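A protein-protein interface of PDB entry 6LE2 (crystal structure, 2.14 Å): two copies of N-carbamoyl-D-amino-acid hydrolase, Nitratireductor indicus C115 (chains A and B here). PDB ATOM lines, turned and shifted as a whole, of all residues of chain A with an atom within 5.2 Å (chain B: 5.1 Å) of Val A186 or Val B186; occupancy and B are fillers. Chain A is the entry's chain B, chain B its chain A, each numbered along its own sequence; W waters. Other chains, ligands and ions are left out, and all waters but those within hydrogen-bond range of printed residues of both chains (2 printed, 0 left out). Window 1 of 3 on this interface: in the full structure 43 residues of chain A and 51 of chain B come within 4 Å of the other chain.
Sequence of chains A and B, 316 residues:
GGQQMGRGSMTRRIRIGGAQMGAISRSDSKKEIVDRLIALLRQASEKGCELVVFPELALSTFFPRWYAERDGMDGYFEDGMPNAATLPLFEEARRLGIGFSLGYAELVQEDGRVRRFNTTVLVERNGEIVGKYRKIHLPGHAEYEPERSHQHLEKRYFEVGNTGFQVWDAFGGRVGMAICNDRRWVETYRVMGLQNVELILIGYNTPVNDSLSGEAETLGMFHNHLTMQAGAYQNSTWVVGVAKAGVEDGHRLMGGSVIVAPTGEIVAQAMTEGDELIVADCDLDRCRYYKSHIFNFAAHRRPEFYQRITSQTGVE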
ATOM      1  N   ARG A 184     -11.952 -15.990   1.224  1.00  0.00           N
ATOM      2  CA  ARG A 184     -11.874 -17.164   2.086  1.00  0.00           C
ATOM      3  C   ARG A 184     -11.283 -16.863   3.463  1.00  0.00           C
ATOM      4  O   ARG A 184     -11.267 -17.755   4.312  1.00  0.00           O
ATOM      5  CB  ARG A 184     -11.072 -18.284   1.406  1.00  0.00           C
ATOM      6  CG  ARG A 184      -9.555 -18.106   1.391  1.00  0.00           C
ATOM      7  CD  ARG A 184      -8.871 -19.394   0.937  1.00  0.00           C
ATOM      8  NE  ARG A 184      -9.353 -19.809  -0.379  1.00  0.00           N
ATOM      9  CZ  ARG A 184      -8.588 -19.941  -1.458  1.00  0.00           C
ATOM     10  NH1 ARG A 184      -9.136 -20.305  -2.611  1.00  0.00           N
ATOM     11  NH2 ARG A 184      -7.277 -19.729  -1.385  1.00  0.00           N
ATOM     12  N   TRP A 185     -10.813 -15.639   3.719  1.00  0.00           N
ATOM     13  CA  TRP A 185     -10.217 -15.290   5.010  1.00  0.00           C
ATOM     14  C   TRP A 185     -11.246 -14.564   5.866  1.00  0.00           C
ATOM     15  O   TRP A 185     -11.763 -13.521   5.456  1.00  0.00           O
ATOM     16  CB  TRP A 185      -8.964 -14.433   4.809  1.00  0.00           C
ATOM     17  CG  TRP A 185      -7.938 -15.201   4.056  1.00  0.00           C
ATOM     18  CD1 TRP A 185      -7.649 -15.100   2.728  1.00  0.00           C
ATOM     19  CD2 TRP A 185      -7.129 -16.269   4.567  1.00  0.00           C
ATOM     20  NE1 TRP A 185      -6.686 -16.018   2.384  1.00  0.00           N
ATOM     21  CE2 TRP A 185      -6.347 -16.747   3.496  1.00  0.00           C
ATOM     22  CE3 TRP A 185      -6.977 -16.855   5.834  1.00  0.00           C
ATOM     23  CZ2 TRP A 185      -5.430 -17.790   3.650  1.00  0.00           C
ATOM     24  CZ3 TRP A 185      -6.066 -17.887   5.991  1.00  0.00           C
ATOM     25  CH2 TRP A 185      -5.299 -18.342   4.901  1.00  0.00           C
ATOM     26  N   VAL A 186     -11.548 -15.107   7.052  1.00  0.00           N
ATOM     27  CA  VAL A 186     -12.540 -14.434   7.898  1.00  0.00           C
ATOM     28  C   VAL A 186     -12.112 -12.997   8.183  1.00  0.00           C
ATOM     29  O   VAL A 186     -12.962 -12.106   8.307  1.00  0.00           O
ATOM     30  CB  VAL A 186     -12.804 -15.218   9.206  1.00  0.00           C
ATOM     31  CG1 VAL A 186     -13.344 -16.616   8.920  1.00  0.00           C
ATOM     32  CG2 VAL A 186     -11.549 -15.283  10.098  1.00  0.00           C
ATOM     33  N   GLU A 187     -10.798 -12.736   8.223  1.00  0.00           N
ATOM     34  CA  GLU A 187     -10.299 -11.400   8.548  1.00  0.00           C
ATOM     35  C   GLU A 187     -10.775 -10.361   7.539  1.00  0.00           C
ATOM     36  O   GLU A 187     -11.025  -9.204   7.896  1.00  0.00           O
ATOM     37  CB  GLU A 187      -8.776 -11.416   8.604  1.00  0.00           C
ATOM     38  CG  GLU A 187      -8.197 -12.179   9.763  1.00  0.00           C
ATOM     39  CD  GLU A 187      -7.957 -13.664   9.468  1.00  0.00           C
ATOM     40  OE1 GLU A 187      -8.517 -14.182   8.478  1.00  0.00           O
ATOM     41  OE2 GLU A 187      -7.227 -14.313  10.256  1.00  0.00           O
ATOM     42  N   THR A 188     -10.897 -10.761   6.276  1.00  0.00           N
ATOM     43  CA  THR A 188     -11.299  -9.841   5.219  1.00  0.00           C
ATOM     44  C   THR A 188     -12.636  -9.180   5.538  1.00  0.00           C
ATOM     45  O   THR A 188     -12.767  -7.952   5.466  1.00  0.00           O
ATOM     46  CB  THR A 188     -11.380 -10.586   3.884  1.00  0.00           C
ATOM     47  OG1 THR A 188     -10.061 -10.877   3.412  1.00  0.00           O
ATOM     48  CG2 THR A 188     -12.111  -9.744   2.842  1.00  0.00           C
ATOM     49  N   TYR A 189     -13.641  -9.979   5.894  1.00  0.00           N
ATOM     50  CA  TYR A 189     -14.944  -9.411   6.230  1.00  0.00           C
ATOM     51  C   TYR A 189     -14.941  -8.768   7.609  1.00  0.00           C
ATOM     52  O   TYR A 189     -15.629  -7.763   7.816  1.00  0.00           O
ATOM     53  CB  TYR A 189     -16.050 -10.467   6.191  1.00  0.00           C
ATOM     54  CG  TYR A 189     -16.064 -11.376   4.983  1.00  0.00           C
ATOM     55  CD1 TYR A 189     -15.291 -12.541   4.953  1.00  0.00           C
ATOM     56  CD2 TYR A 189     -16.873 -11.094   3.887  1.00  0.00           C
ATOM     57  CE1 TYR A 189     -15.317 -13.394   3.847  1.00  0.00           C
ATOM     58  CE2 TYR A 189     -16.909 -11.937   2.777  1.00  0.00           C
ATOM     59  CZ  TYR A 189     -16.126 -13.085   2.770  1.00  0.00           C
ATOM     60  OH  TYR A 189     -16.158 -13.917   1.690  1.00  0.00           O
ATOM     61  N   ARG A 190     -14.189  -9.326   8.561  1.00  0.00           N
ATOM     62  CA  ARG A 190     -14.205  -8.752   9.899  1.00  0.00           C
ATOM     63  C   ARG A 190     -13.617  -7.348   9.905  1.00  0.00           C
ATOM     64  O   ARG A 190     -14.174  -6.450  10.543  1.00  0.00           O
ATOM     65  CB  ARG A 190     -13.453  -9.637  10.888  1.00  0.00           C
ATOM     66  CG  ARG A 190     -13.505  -9.094  12.310  1.00  0.00           C
ATOM     67  CD  ARG A 190     -14.935  -8.904  12.772  1.00  0.00           C
ATOM     68  NE  ARG A 190     -15.331  -9.985  13.660  1.00  0.00           N
ATOM     69  CZ  ARG A 190     -16.527 -10.562  13.652  1.00  0.00           C
ATOM     70  NH1 ARG A 190     -17.441 -10.151  12.782  1.00  0.00           N
ATOM     71  NH2 ARG A 190     -16.796 -11.557  14.504  1.00  0.00           N
ATOM     72  N   VAL A 191     -12.499  -7.143   9.194  1.00  0.00           N
ATOM     73  CA  VAL A 191     -11.856  -5.829   9.151  1.00  0.00           C
ATOM     74  C   VAL A 191     -12.834  -4.776   8.648  1.00  0.00           C
ATOM     75  O   VAL A 191     -12.866  -3.645   9.150  1.00  0.00           O
ATOM     76  CB  VAL A 191     -10.580  -5.876   8.285  1.00  0.00           C
ATOM     77  CG1 VAL A 191     -10.041  -4.482   8.041  1.00  0.00           C
ATOM     78  CG2 VAL A 191      -9.503  -6.707   8.961  1.00  0.00           C
ATOM     79  N   GLN A 234     -22.117 -12.954   9.457  1.00  0.00           N
ATOM     80  CA  GLN A 234     -21.346 -12.695  10.672  1.00  0.00           C
ATOM     81  C   GLN A 234     -20.902 -11.240  10.803  1.00  0.00           C
ATOM     82  O   GLN A 234     -20.477 -10.824  11.889  1.00  0.00           O
ATOM     83  CB  GLN A 234     -20.144 -13.640  10.747  1.00  0.00           C
ATOM     84  CG  GLN A 234     -20.536 -15.058  11.186  1.00  0.00           C
ATOM     85  CD  GLN A 234     -19.383 -16.055  11.129  1.00  0.00           C
ATOM     86  OE1 GLN A 234     -18.798 -16.290  10.066  1.00  0.00           O
ATOM     87  NE2 GLN A 234     -19.041 -16.630  12.283  1.00  0.00           N
ATOM     88  N   ARG B 184     -20.786 -17.929  17.095  1.00  0.00           N
ATOM     89  CA  ARG B 184     -21.132 -16.859  16.166  1.00  0.00           C
ATOM     90  C   ARG B 184     -19.963 -15.945  15.823  1.00  0.00           C
ATOM     91  O   ARG B 184     -20.121 -15.090  14.948  1.00  0.00           O
ATOM     92  CB  ARG B 184     -22.238 -15.976  16.755  1.00  0.00           C
ATOM     93  CG  ARG B 184     -23.597 -16.609  16.820  1.00  0.00           C
ATOM     94  CD  ARG B 184     -24.687 -15.555  16.664  1.00  0.00           C
ATOM     95  NE  ARG B 184     -24.868 -14.764  17.876  1.00  0.00           N
ATOM     96  CZ  ARG B 184     -25.654 -15.134  18.885  1.00  0.00           C
ATOM     97  NH1 ARG B 184     -26.318 -16.285  18.818  1.00  0.00           N
ATOM     98  NH2 ARG B 184     -25.775 -14.358  19.961  1.00  0.00           N
ATOM     99  N   TRP B 185     -18.828 -16.066  16.513  1.00  0.00           N
ATOM    100  CA  TRP B 185     -17.701 -15.145  16.397  1.00  0.00           C
ATOM    101  C   TRP B 185     -16.570 -15.812  15.630  1.00  0.00           C
ATOM    102  O   TRP B 185     -16.035 -16.831  16.085  1.00  0.00           O
ATOM    103  CB  TRP B 185     -17.205 -14.726  17.779  1.00  0.00           C
ATOM    104  CG  TRP B 185     -18.226 -13.960  18.538  1.00  0.00           C
ATOM    105  CD1 TRP B 185     -19.164 -14.461  19.387  1.00  0.00           C
ATOM    106  CD2 TRP B 185     -18.434 -12.552  18.494  1.00  0.00           C
ATOM    107  NE1 TRP B 185     -19.953 -13.449  19.871  1.00  0.00           N
ATOM    108  CE2 TRP B 185     -19.521 -12.264  19.341  1.00  0.00           C
ATOM    109  CE3 TRP B 185     -17.811 -11.504  17.815  1.00  0.00           C
ATOM    110  CZ2 TRP B 185     -19.989 -10.977  19.537  1.00  0.00           C
ATOM    111  CZ3 TRP B 185     -18.285 -10.228  18.001  1.00  0.00           C
ATOM    112  CH2 TRP B 185     -19.359  -9.970  18.859  1.00  0.00           C
ATOM    113  N   VAL B 186     -16.176 -15.227  14.491  1.00  0.00           N
ATOM    114  CA  VAL B 186     -15.101 -15.851  13.709  1.00  0.00           C
ATOM    115  C   VAL B 186     -13.817 -15.920  14.525  1.00  0.00           C
ATOM    116  O   VAL B 186     -12.980 -16.803  14.296  1.00  0.00           O
ATOM    117  CB  VAL B 186     -14.861 -15.130  12.366  1.00  0.00           C
ATOM    118  CG1 VAL B 186     -16.149 -15.089  11.517  1.00  0.00           C
ATOM    119  CG2 VAL B 186     -14.284 -13.735  12.587  1.00  0.00           C
ATOM    120  N   GLU B 187     -13.660 -15.019  15.509  1.00  0.00           N
ATOM    121  CA  GLU B 187     -12.453 -14.994  16.332  1.00  0.00           C
ATOM    122  C   GLU B 187     -12.323 -16.253  17.167  1.00  0.00           C
ATOM    123  O   GLU B 187     -11.197 -16.692  17.451  1.00  0.00           O
ATOM    124  CB  GLU B 187     -12.453 -13.769  17.262  1.00  0.00           C
ATOM    125  CG  GLU B 187     -12.360 -12.421  16.558  1.00  0.00           C
ATOM    126  CD  GLU B 187     -13.703 -11.868  16.126  1.00  0.00           C
ATOM    127  OE1 GLU B 187     -14.707 -12.637  16.125  1.00  0.00           O
ATOM    128  OE2 GLU B 187     -13.743 -10.659  15.791  1.00  0.00           O
ATOM    129  N   THR B 188     -13.458 -16.824  17.587  1.00  0.00           N
ATOM    130  CA  THR B 188     -13.445 -18.052  18.375  1.00  0.00           C
ATOM    131  C   THR B 188     -12.718 -19.163  17.645  1.00  0.00           C
ATOM    132  O   THR B 188     -11.796 -19.784  18.190  1.00  0.00           O
ATOM    133  CB  THR B 188     -14.871 -18.495  18.680  1.00  0.00           C
ATOM    134  OG1 THR B 188     -15.500 -17.527  19.521  1.00  0.00           O
ATOM    135  CG2 THR B 188     -14.851 -19.832  19.378  1.00  0.00           C
ATOM    136  N   TYR B 189     -13.139 -19.450  16.412  1.00  0.00           N
ATOM    137  CA  TYR B 189     -12.497 -20.518  15.652  1.00  0.00           C
ATOM    138  C   TYR B 189     -11.064 -20.145  15.281  1.00  0.00           C
ATOM    139  O   TYR B 189     -10.148 -20.964  15.430  1.00  0.00           O
ATOM    140  CB  TYR B 189     -13.306 -20.830  14.394  1.00  0.00           C
ATOM    141  CG  TYR B 189     -14.793 -21.072  14.604  1.00  0.00           C
ATOM    142  CD1 TYR B 189     -15.694 -20.009  14.615  1.00  0.00           C
ATOM    143  CD2 TYR B 189     -15.295 -22.357  14.759  1.00  0.00           C
ATOM    144  CE1 TYR B 189     -17.056 -20.220  14.787  1.00  0.00           C
ATOM    145  CE2 TYR B 189     -16.663 -22.583  14.930  1.00  0.00           C
ATOM    146  CZ  TYR B 189     -17.538 -21.508  14.943  1.00  0.00           C
ATOM    147  OH  TYR B 189     -18.897 -21.706  15.113  1.00  0.00           O
ATOM    148  N   ARG B 190     -10.849 -18.903  14.824  1.00  0.00           N
ATOM    149  CA  ARG B 190      -9.532 -18.504  14.337  1.00  0.00           C
ATOM    150  C   ARG B 190      -8.480 -18.556  15.439  1.00  0.00           C
ATOM    151  O   ARG B 190      -7.341 -18.974  15.194  1.00  0.00           O
ATOM    152  CB  ARG B 190      -9.581 -17.099  13.734  1.00  0.00           C
ATOM    153  CG  ARG B 190      -8.238 -16.622  13.158  1.00  0.00           C
ATOM    154  CD  ARG B 190      -7.754 -17.530  12.017  1.00  0.00           C
ATOM    155  NE  ARG B 190      -8.009 -16.989  10.681  1.00  0.00           N
ATOM    156  CZ  ARG B 190      -8.662 -17.628   9.707  1.00  0.00           C
ATOM    157  NH1 ARG B 190      -9.144 -18.839   9.904  1.00  0.00           N
ATOM    158  NH2 ARG B 190      -8.839 -17.052   8.522  1.00  0.00           N
ATOM    159  N   VAL B 191      -8.829 -18.119  16.651  1.00  0.00           N
ATOM    160  CA  VAL B 191      -7.848 -18.127  17.732  1.00  0.00           C
ATOM    161  C   VAL B 191      -7.362 -19.554  17.998  1.00  0.00           C
ATOM    162  O   VAL B 191      -6.173 -19.780  18.248  1.00  0.00           O
ATOM    163  CB  VAL B 191      -8.423 -17.456  18.995  1.00  0.00           C
ATOM    164  CG1 VAL B 191      -7.572 -17.761  20.201  1.00  0.00           C
ATOM    165  CG2 VAL B 191      -8.488 -15.916  18.803  1.00  0.00           C
ATOM    166  N   GLN B 234     -13.100 -22.903   7.366  1.00  0.00           N
ATOM    167  CA  GLN B 234     -12.101 -21.840   7.274  1.00  0.00           C
ATOM    168  C   GLN B 234     -10.977 -21.975   8.286  1.00  0.00           C
ATOM    169  O   GLN B 234     -10.015 -21.203   8.227  1.00  0.00           O
ATOM    170  CB  GLN B 234     -12.770 -20.471   7.414  1.00  0.00           C
ATOM    171  CG  GLN B 234     -13.640 -20.148   6.209  1.00  0.00           C
ATOM    172  CD  GLN B 234     -14.325 -18.800   6.305  1.00  0.00           C
ATOM    173  OE1 GLN B 234     -15.404 -18.690   6.870  1.00  0.00           O
ATOM    174  NE2 GLN B 234     -13.697 -17.769   5.750  1.00  0.00           N
HETATM  175  O   HOH W   1     -10.124 -18.612   6.595  1.00  0.00           O
HETATM  176  O   HOH W   2     -19.330 -12.688  13.996  1.00  0.00           O
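OE2 of Glu B187 lies within salt-bridge range of NE of Arg A190, at 2.7 Å.
NE2 of Gln B234 sits at hydrogen-bond distance from O of Arg A184 (2.8 Å).
The side-chain amide nitrogen (NE2) of Gln A234 lies within hydrogen-bond range of the backbone carbonyl oxygen (O) of Arg B184, at 3.3 Å.
NE of Arg B190 is in salt-bridge range of OE2 of Glu A187, 2.8 Å away.
The guanidinium group of Arg A190 is in hydrogen-bond range of the backbone carbonyl oxygen of Gln A234 (3.2 Å).
NH1 of Arg B190 lies within hydrogen-bond range of O of Gln B234 (3.0 Å).
Trp A185 touches Arg B190.
Val B186 touches Val A186.
NH2 of Arg B190 touches CG2 of Val A186, at 3.6 Å.
Val A186 touches Gln B234 (CG1 to NE2, 3.4 Å).
Arg A190 touches Trp B185 (NH2 to CE3, 3.5 Å).
Arg A190 touches Val B186.
Gln A234 touches Val B186 (OE1 to CG1, 3.3 Å).
Val A186 touches just these residues of chain B: Val B186, Arg B190 and Gln B234.
Of chain A, only Val A186, Arg A190 and Gln A234 come within 4 Å of Val B186.
Printed residues of chain A within 4 Å of Arg B190: Trp A185, Val A186 and Glu A187.
Printed residues of chain A within 4 Å of Trp B185: Arg A190.
Of the printed residues of chain B, Gln A234 touches Arg B184 (3.3 Å) and Val B186 (3.3 Å).
Tyr B189 touches none of the printed residues of chain A.
The nearest printed residue of chain B that does not touch Val A186 is Glu B187 (5.8 Å).
The nearest printed residue of chain A that does not touch Val B186 is Glu A187 (5.7 Å).
Printed residues of chain B that touch a printed residue of chain A: Arg B184, Trp B185, Val B186, Glu B187, Arg B190 and Gln B234.
Of the 9 printed residues of chain A, 6 touch a printed residue of chain B.
Hydrophobic or aromatic side chains of chain A within 4 Å of the printed part of chain B: Trp A185 and Val A186.
Arg A184 touches Gln B234, and with the chains exchanged Gln A234 touches Arg B184.
Trp A185 touches Arg B190, and with the chains exchanged Arg A190 touches Trp B185.
Val A186 touches Arg B190, and with the chains exchanged Arg A190 touches Val B186.
Val A186 touches Gln B234, and with the chains exchanged Gln A234 touches Val B186.
Of the 11 pairs that touch across the chains among the printed residues, 11 have their exchanged pair printed and touching as well.
Water W1 lies within hydrogen-bond range of the backbone carbonyl oxygen (O) of Arg A184 (2.7 Å), the guanidinium group (NH2) of Arg B190 (2.8 Å) and the backbone carbonyl oxygen (O) of Gln B234 (3.1 Å).
Water W2 lies within hydrogen-bond range of the backbone carbonyl oxygen of Arg B184, the guanidinium group of Arg A190 and the backbone carbonyl oxygen of Gln A234.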
